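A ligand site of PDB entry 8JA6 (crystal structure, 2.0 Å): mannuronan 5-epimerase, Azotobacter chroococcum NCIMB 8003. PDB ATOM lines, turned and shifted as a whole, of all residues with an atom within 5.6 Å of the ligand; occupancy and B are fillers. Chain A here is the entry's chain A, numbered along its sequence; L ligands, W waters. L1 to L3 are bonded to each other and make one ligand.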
ATOM      1  N   GLU A  51      -3.158 -13.450   6.191  1.00  0.00           N
ATOM      2  CA  GLU A  51      -4.351 -12.751   5.760  1.00  0.00           C
ATOM      3  C   GLU A  51      -4.429 -11.382   6.427  1.00  0.00           C
ATOM      4  O   GLU A  51      -3.809 -11.145   7.476  1.00  0.00           O
ATOM      5  CB  GLU A  51      -5.623 -13.546   6.091  1.00  0.00           C
ATOM      6  CG  GLU A  51      -5.472 -15.019   5.840  1.00  0.00           C
ATOM      7  CD  GLU A  51      -6.627 -15.598   5.072  1.00  0.00           C
ATOM      8  OE1 GLU A  51      -6.368 -16.343   4.099  1.00  0.00           O
ATOM      9  OE2 GLU A  51      -7.779 -15.290   5.437  1.00  0.00           O
ATOM     10  N   ALA A  52      -5.198 -10.499   5.794  1.00  0.00           N
ATOM     11  CA  ALA A  52      -5.380  -9.150   6.307  1.00  0.00           C
ATOM     12  C   ALA A  52      -5.917  -9.163   7.729  1.00  0.00           C
ATOM     13  O   ALA A  52      -5.504  -8.335   8.555  1.00  0.00           O
ATOM     14  CB  ALA A  52      -6.325  -8.366   5.394  1.00  0.00           C
ATOM     15  N   SER A  53      -6.825 -10.091   8.041  1.00  0.00           N
ATOM     16  CA  SER A  53      -7.450 -10.135   9.365  1.00  0.00           C
ATOM     17  C   SER A  53      -6.493 -10.626  10.437  1.00  0.00           C
ATOM     18  O   SER A  53      -6.849 -10.626  11.624  1.00  0.00           O
ATOM     19  CB  SER A  53      -8.707 -11.007   9.328  1.00  0.00           C
ATOM     20  OG  SER A  53      -8.374 -12.372   9.121  1.00  0.00           O
ATOM     21  N   ASP A  54      -5.292 -11.067  10.059  1.00  0.00           N
ATOM     22  CA  ASP A  54      -4.286 -11.390  11.056  1.00  0.00           C
ATOM     23  C   ASP A  54      -3.606 -10.148  11.598  1.00  0.00           C
ATOM     24  O   ASP A  54      -2.981 -10.216  12.667  1.00  0.00           O
ATOM     25  CB  ASP A  54      -3.244 -12.357  10.464  1.00  0.00           C
ATOM     26  CG  ASP A  54      -3.839 -13.714  10.133  1.00  0.00           C
ATOM     27  OD1 ASP A  54      -4.835 -14.116  10.784  1.00  0.00           O
ATOM     28  OD2 ASP A  54      -3.325 -14.377   9.210  1.00  0.00           O
ATOM     29  N   LYS A  84      -2.581  -6.247   2.181  1.00  0.00           N
ATOM     30  CA  LYS A  84      -3.516  -5.541   3.052  1.00  0.00           C
ATOM     31  C   LYS A  84      -3.368  -6.041   4.482  1.00  0.00           C
ATOM     32  O   LYS A  84      -3.340  -7.247   4.718  1.00  0.00           O
ATOM     33  CB  LYS A  84      -4.941  -5.742   2.554  1.00  0.00           C
ATOM     34  CG  LYS A  84      -5.978  -4.960   3.361  1.00  0.00           C
ATOM     35  CD  LYS A  84      -7.354  -5.602   3.317  1.00  0.00           C
ATOM     36  CE  LYS A  84      -8.316  -4.793   2.457  1.00  0.00           C
ATOM     37  NZ  LYS A  84      -9.699  -4.869   3.013  1.00  0.00           N
ATOM     38  N   THR A  86      -4.956  -5.324   8.232  1.00  0.00           N
ATOM     39  CA  THR A  86      -6.049  -4.689   8.959  1.00  0.00           C
ATOM     40  C   THR A  86      -5.732  -4.676  10.465  1.00  0.00           C
ATOM     41  O   THR A  86      -6.229  -5.501  11.238  1.00  0.00           O
ATOM     42  CB  THR A  86      -7.366  -5.401   8.667  1.00  0.00           C
ATOM     43  OG1 THR A  86      -7.526  -5.545   7.251  1.00  0.00           O
ATOM     44  CG2 THR A  86      -8.559  -4.618   9.257  1.00  0.00           C
ATOM     45  N   ARG A  90      -4.210  -5.366  16.803  1.00  0.00           N
ATOM     46  CA  ARG A  90      -5.623  -5.651  16.657  1.00  0.00           C
ATOM     47  C   ARG A  90      -6.041  -6.768  17.603  1.00  0.00           C
ATOM     48  O   ARG A  90      -5.199  -7.528  18.105  1.00  0.00           O
ATOM     49  CB  ARG A  90      -5.961  -6.027  15.206  1.00  0.00           C
ATOM     50  CG  ARG A  90      -5.602  -7.470  14.817  1.00  0.00           C
ATOM     51  CD  ARG A  90      -6.262  -7.860  13.496  1.00  0.00           C
ATOM     52  NE  ARG A  90      -7.649  -8.246  13.676  1.00  0.00           N
ATOM     53  CZ  ARG A  90      -8.591  -8.131  12.757  1.00  0.00           C
ATOM     54  NH1 ARG A  90      -8.328  -7.615  11.562  1.00  0.00           N
ATOM     55  NH2 ARG A  90      -9.828  -8.538  13.033  1.00  0.00           N
ATOM     56  N   ASN A  93     -10.729 -11.282  15.241  1.00  0.00           N
ATOM     57  CA  ASN A  93     -12.057 -11.448  14.689  1.00  0.00           C
ATOM     58  C   ASN A  93     -12.739 -12.671  15.296  1.00  0.00           C
ATOM     59  O   ASN A  93     -12.127 -13.735  15.455  1.00  0.00           O
ATOM     60  CB  ASN A  93     -11.936 -11.620  13.171  1.00  0.00           C
ATOM     61  CG  ASN A  93     -13.270 -11.708  12.473  1.00  0.00           C
ATOM     62  OD1 ASN A  93     -14.056 -12.631  12.692  1.00  0.00           O
ATOM     63  ND2 ASN A  93     -13.541 -10.731  11.613  1.00  0.00           N
ATOM     64  N   ASP A 119      -4.159  -0.445   8.444  1.00  0.00           N
ATOM     65  CA  ASP A 119      -4.817   0.256   9.540  1.00  0.00           C
ATOM     66  C   ASP A 119      -3.984   0.093  10.803  1.00  0.00           C
ATOM     67  O   ASP A 119      -3.325  -0.942  10.987  1.00  0.00           O
ATOM     68  CB  ASP A 119      -6.231  -0.278   9.745  1.00  0.00           C
ATOM     69  CG  ASP A 119      -7.008  -0.357   8.430  1.00  0.00           C
ATOM     70  OD1 ASP A 119      -7.205   0.714   7.804  1.00  0.00           O
ATOM     71  OD2 ASP A 119      -7.386  -1.471   8.014  1.00  0.00           O
ATOM     72  N   TYR A 122      -7.049  -1.802  15.341  1.00  0.00           N
ATOM     73  CA  TYR A 122      -8.337  -2.366  14.925  1.00  0.00           C
ATOM     74  C   TYR A 122      -8.921  -3.195  16.063  1.00  0.00           C
ATOM     75  O   TYR A 122      -8.206  -3.983  16.695  1.00  0.00           O
ATOM     76  CB  TYR A 122      -8.158  -3.225  13.664  1.00  0.00           C
ATOM     77  CG  TYR A 122      -9.440  -3.668  12.997  1.00  0.00           C
ATOM     78  CD1 TYR A 122     -10.036  -4.862  13.344  1.00  0.00           C
ATOM     79  CD2 TYR A 122     -10.035  -2.903  11.998  1.00  0.00           C
ATOM     80  CE1 TYR A 122     -11.215  -5.284  12.740  1.00  0.00           C
ATOM     81  CE2 TYR A 122     -11.216  -3.323  11.371  1.00  0.00           C
ATOM     82  CZ  TYR A 122     -11.792  -4.513  11.748  1.00  0.00           C
ATOM     83  OH  TYR A 122     -12.956  -4.959  11.157  1.00  0.00           O
ATOM     84  N   ILE A 126     -17.327  -9.153  15.060  1.00  0.00           N
ATOM     85  CA  ILE A 126     -17.633  -9.687  13.729  1.00  0.00           C
ATOM     86  C   ILE A 126     -18.578  -8.703  13.060  1.00  0.00           C
ATOM     87  O   ILE A 126     -19.674  -8.461  13.578  1.00  0.00           O
ATOM     88  CB  ILE A 126     -18.297 -11.075  13.767  1.00  0.00           C
ATOM     89  CG1 ILE A 126     -17.402 -12.159  14.360  1.00  0.00           C
ATOM     90  CG2 ILE A 126     -18.692 -11.492  12.357  1.00  0.00           C
ATOM     91  CD1 ILE A 126     -18.168 -13.412  14.735  1.00  0.00           C
ATOM     92  N   PRO A 127     -18.224  -8.134  11.903  1.00  0.00           N
ATOM     93  CA  PRO A 127     -19.164  -7.242  11.213  1.00  0.00           C
ATOM     94  C   PRO A 127     -20.510  -7.923  11.001  1.00  0.00           C
ATOM     95  O   PRO A 127     -20.579  -9.074  10.597  1.00  0.00           O
ATOM     96  CB  PRO A 127     -18.471  -6.936   9.890  1.00  0.00           C
ATOM     97  CG  PRO A 127     -17.005  -7.016  10.227  1.00  0.00           C
ATOM     98  CD  PRO A 127     -16.904  -8.143  11.261  1.00  0.00           C
ATOM     99  N   ARG A 128     -21.587  -7.210  11.370  1.00  0.00           N
ATOM    100  CA  ARG A 128     -22.993  -7.581  11.157  1.00  0.00           C
ATOM    101  C   ARG A 128     -23.517  -8.677  12.072  1.00  0.00           C
ATOM    102  O   ARG A 128     -24.576  -9.244  11.793  1.00  0.00           O
ATOM    103  CB  ARG A 128     -23.236  -8.002   9.704  1.00  0.00           C
ATOM    104  CG  ARG A 128     -23.402  -6.832   8.776  1.00  0.00           C
ATOM    105  CD  ARG A 128     -22.837  -7.151   7.401  1.00  0.00           C
ATOM    106  NE  ARG A 128     -21.992  -6.056   6.954  1.00  0.00           N
ATOM    107  CZ  ARG A 128     -20.749  -6.195   6.521  1.00  0.00           C
ATOM    108  NH1 ARG A 128     -20.165  -7.379   6.439  1.00  0.00           N
ATOM    109  NH2 ARG A 128     -20.058  -5.103   6.163  1.00  0.00           N
ATOM    110  N   ARG A 148      -4.242   3.551   5.304  1.00  0.00           N
ATOM    111  CA  ARG A 148      -5.661   3.876   5.377  1.00  0.00           C
ATOM    112  C   ARG A 148      -6.107   4.544   6.688  1.00  0.00           C
ATOM    113  O   ARG A 148      -6.022   5.763   6.803  1.00  0.00           O
ATOM    114  CB  ARG A 148      -6.476   2.601   5.142  1.00  0.00           C
ATOM    115  CG  ARG A 148      -7.899   2.821   4.712  1.00  0.00           C
ATOM    116  CD  ARG A 148      -8.519   1.520   4.210  1.00  0.00           C
ATOM    117  NE  ARG A 148      -8.654   0.535   5.273  1.00  0.00           N
ATOM    118  CZ  ARG A 148      -9.553  -0.451   5.278  1.00  0.00           C
ATOM    119  NH1 ARG A 148     -10.411  -0.602   4.281  1.00  0.00           N
ATOM    120  NH2 ARG A 148      -9.589  -1.297   6.306  1.00  0.00           N
ATOM    121  N   TYR A 149      -6.354   3.769   7.740  1.00  0.00           N
ATOM    122  CA  TYR A 149      -7.055   4.274   8.920  1.00  0.00           C
ATOM    123  C   TYR A 149      -6.120   4.184  10.110  1.00  0.00           C
ATOM    124  O   TYR A 149      -5.633   3.090  10.422  1.00  0.00           O
ATOM    125  CB  TYR A 149      -8.349   3.501   9.202  1.00  0.00           C
ATOM    126  CG  TYR A 149      -9.449   3.609   8.170  1.00  0.00           C
ATOM    127  CD1 TYR A 149      -9.772   4.816   7.578  1.00  0.00           C
ATOM    128  CD2 TYR A 149     -10.180   2.476   7.791  1.00  0.00           C
ATOM    129  CE1 TYR A 149     -10.788   4.916   6.630  1.00  0.00           C
ATOM    130  CE2 TYR A 149     -11.199   2.562   6.834  1.00  0.00           C
ATOM    131  CZ  TYR A 149     -11.492   3.792   6.261  1.00  0.00           C
ATOM    132  OH  TYR A 149     -12.497   3.886   5.319  1.00  0.00           O
ATOM    133  N   ASP A 152      -8.735   2.650  14.156  1.00  0.00           N
ATOM    134  CA  ASP A 152      -9.875   2.053  13.455  1.00  0.00           C
ATOM    135  C   ASP A 152     -10.643   1.080  14.344  1.00  0.00           C
ATOM    136  O   ASP A 152     -10.879  -0.066  13.966  1.00  0.00           O
ATOM    137  CB  ASP A 152      -9.369   1.359  12.188  1.00  0.00           C
ATOM    138  CG  ASP A 152     -10.481   0.961  11.228  1.00  0.00           C
ATOM    139  OD1 ASP A 152     -11.623   1.429  11.357  1.00  0.00           O
ATOM    140  OD2 ASP A 152     -10.189   0.165  10.305  1.00  0.00           O
ATOM    141  N   HIS A 154     -13.620  -0.955  15.715  1.00  0.00           N
ATOM    142  CA  HIS A 154     -14.568  -1.446  14.727  1.00  0.00           C
ATOM    143  C   HIS A 154     -15.674  -2.241  15.400  1.00  0.00           C
ATOM    144  O   HIS A 154     -15.741  -2.349  16.629  1.00  0.00           O
ATOM    145  CB  HIS A 154     -13.841  -2.268  13.646  1.00  0.00           C
ATOM    146  CG  HIS A 154     -14.407  -2.108  12.267  1.00  0.00           C
ATOM    147  ND1 HIS A 154     -15.390  -2.943  11.783  1.00  0.00           N
ATOM    148  CD2 HIS A 154     -14.115  -1.237  11.280  1.00  0.00           C
ATOM    149  CE1 HIS A 154     -15.690  -2.571  10.551  1.00  0.00           C
ATOM    150  NE2 HIS A 154     -14.931  -1.542  10.216  1.00  0.00           N
ATOM    151  N   GLU A 155     -16.557  -2.795  14.568  1.00  0.00           N
ATOM    152  CA  GLU A 155     -17.852  -3.293  14.996  1.00  0.00           C
ATOM    153  C   GLU A 155     -17.743  -4.625  15.735  1.00  0.00           C
ATOM    154  O   GLU A 155     -17.079  -5.548  15.256  1.00  0.00           O
ATOM    155  CB  GLU A 155     -18.755  -3.432  13.775  1.00  0.00           C
ATOM    156  CG  GLU A 155     -20.054  -4.161  13.999  1.00  0.00           C
ATOM    157  CD  GLU A 155     -20.889  -4.249  12.728  1.00  0.00           C
ATOM    158  OE1 GLU A 155     -22.039  -4.727  12.801  1.00  0.00           O
ATOM    159  OE2 GLU A 155     -20.393  -3.834  11.661  1.00  0.00           O
ATOM    160  N   ASP A 178     -16.227   2.756  14.096  1.00  0.00           N
ATOM    161  CA  ASP A 178     -17.239   1.940  13.460  1.00  0.00           C
ATOM    162  C   ASP A 178     -18.002   1.140  14.512  1.00  0.00           C
ATOM    163  O   ASP A 178     -17.411   0.276  15.185  1.00  0.00           O
ATOM    164  CB  ASP A 178     -16.526   1.035  12.460  1.00  0.00           C
ATOM    165  CG  ASP A 178     -17.423   0.467  11.435  1.00  0.00           C
ATOM    166  OD1 ASP A 178     -17.957  -0.608  11.713  1.00  0.00           O
ATOM    167  OD2 ASP A 178     -17.561   1.072  10.342  1.00  0.00           O
HETATM  168  C1  LIG L   1     -11.760 -16.451   9.120  1.00  0.00           C
HETATM  169  C2  LIG L   1     -10.815 -15.326   9.596  1.00  0.00           C
HETATM  170  O1  LIG L   1      -9.769 -15.007   8.730  1.00  0.00           O
HETATM  171  C3  LIG L   1     -11.724 -14.056   9.725  1.00  0.00           C
HETATM  172  O2  LIG L   1     -10.962 -12.956  10.081  1.00  0.00           O
HETATM  173  C4  LIG L   1     -12.426 -13.698   8.384  1.00  0.00           C
HETATM  174  O3  LIG L   1     -13.370 -12.710   8.623  1.00  0.00           O
HETATM  175  C5  LIG L   1     -13.185 -14.986   8.009  1.00  0.00           C
HETATM  176  O4  LIG L   1     -12.319 -16.094   7.877  1.00  0.00           O
HETATM  177  C6  LIG L   1     -13.752 -14.801   6.579  1.00  0.00           C
HETATM  178  O5  LIG L   1     -14.920 -14.277   6.605  1.00  0.00           O
HETATM  179  O6  LIG L   1     -13.079 -15.139   5.627  1.00  0.00           O
HETATM  180  O7  LIG L   1     -11.054 -17.637   8.857  1.00  0.00           O
HETATM  181  C1  LG2 L   2     -13.011 -11.427   8.082  1.00  0.00           C
HETATM  182  C2  LG2 L   2     -14.332 -10.754   7.689  1.00  0.00           C
HETATM  183  O1  LG2 L   2     -15.251 -10.652   8.735  1.00  0.00           O
HETATM  184  C3  LG2 L   2     -14.003  -9.300   7.194  1.00  0.00           C
HETATM  185  O2  LG2 L   2     -15.193  -8.581   6.950  1.00  0.00           O
HETATM  186  C4  LG2 L   2     -13.164  -8.488   8.214  1.00  0.00           C
HETATM  187  O3  LG2 L   2     -12.640  -7.355   7.603  1.00  0.00           O
HETATM  188  C5  LG2 L   2     -11.953  -9.382   8.532  1.00  0.00           C
HETATM  189  O4  LG2 L   2     -12.332 -10.653   9.028  1.00  0.00           O
HETATM  190  C6  LG2 L   2     -11.149  -8.690   9.699  1.00  0.00           C
HETATM  191  O5  LG2 L   2     -10.169  -7.997   9.252  1.00  0.00           O
HETATM  192  O6  LG2 L   2     -11.483  -8.857  10.858  1.00  0.00           O
HETATM  193  C1  LG3 L   3     -13.351  -6.159   7.962  1.00  0.00           C
HETATM  194  C2  LG3 L   3     -12.381  -5.038   7.609  1.00  0.00           C
HETATM  195  O1  LG3 L   3     -11.874  -5.139   6.313  1.00  0.00           O
HETATM  196  C3  LG3 L   3     -13.135  -3.677   7.719  1.00  0.00           C
HETATM  197  O2  LG3 L   3     -12.315  -2.656   7.256  1.00  0.00           O
HETATM  198  C4  LG3 L   3     -14.442  -3.664   6.886  1.00  0.00           C
HETATM  199  O3  LG3 L   3     -15.133  -2.470   7.098  1.00  0.00           O
HETATM  200  C5  LG3 L   3     -15.245  -4.826   7.492  1.00  0.00           C
HETATM  201  O4  LG3 L   3     -14.566  -6.054   7.250  1.00  0.00           O
HETATM  202  C6  LG3 L   3     -16.595  -4.994   6.728  1.00  0.00           C
HETATM  203  O5  LG3 L   3     -17.575  -4.478   7.378  1.00  0.00           O
HETATM  204  O6  LG3 L   3     -16.625  -5.565   5.653  1.00  0.00           O
HETATM  205  O   HOH W   1      -9.673  -6.841   6.740  1.00  0.00           O
HETATM  206  O   HOH W   2     -12.195  -0.602   8.586  1.00  0.00           O
HETATM  207  O   HOH W   3     -13.724  -7.315  11.359  1.00  0.00           O
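Water W2 lies within hydrogen-bond range of O2 of LG3 L3 (2.4 Å), OD2 of Asp 152 (2.8 Å) and NE2 of His 154 (3.3 Å).
Water W3 lies within hydrogen-bond range of OH of Tyr 122, O6 of LG2 L2 and ND2 of Asn 93.
Water W1 lies within hydrogen-bond range of the side-chain hydroxyl of Thr 86 and an oxygen (O5) of LG2 L2.
O of Ser 53 lies within hydrogen-bond range of NE of Arg 90.
The guanidinium group (NH1) of Arg 90 lies within hydrogen-bond range of the backbone carbonyl oxygen (O) of Thr 86 (3.0 Å).
The backbone NH (N) of Arg 128 sits at hydrogen-bond distance from the side-chain carboxylate (OE1) of Glu 155.
NH2 of Arg 148 lies within salt-bridge range of OD2 of Asp 119 (2.8 Å).
OH of Tyr 122 sits at hydrogen-bond distance from ND1 of His 154.
OD1 of Asp 178 lies close to ND1 of His 154, 3.5 Å away.
The backbone carbonyl oxygen of Ala 52 is in hydrogen-bond range of the backbone NH of Thr 86, 3.1 Å away.
OD2 of Asp 54 is in hydrogen-bond range of N of Glu 51 (3.2 Å).
Glu 51 touches the ligand.
NZ of Lys 84 touches O1 of LG3 L3, at 3.96 Å.
CG2 of Thr 86 touches O5 of LG2 L2 (3.7 Å).
OH of Tyr 122 touches C1 of LG3 L3, at 3.4 Å.
CB of Pro 127 touches O5 of LG3 L3 (3.6 Å).
Of the 19 residues printed, 11 come within 4 Å of the ligand.
The nearest printed residue that does not touch the ligand is Ala 52 (4.7 Å).
O6 of LG2 L2 is in salt-bridge range of NH2 of Arg 90 (2.8 Å).
An oxygen (O2) of LIG L1 is in hydrogen-bond range of the side-chain hydroxyl (OG) of Ser 53, at 2.8 Å.
NH2 of Arg 128 lies within salt-bridge range of O5 of LG3 L3, 2.8 Å away.
An oxygen (O4) of LG2 L2 lies within hydrogen-bond range of the side-chain amide nitrogen of Asn 93.
NH2 of Arg 148 sits at hydrogen-bond distance from O2 of LG3 L3.
An oxygen (O3) of LG3 L3 lies within hydrogen-bond range of a ring nitrogen (NE2) of His 154.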
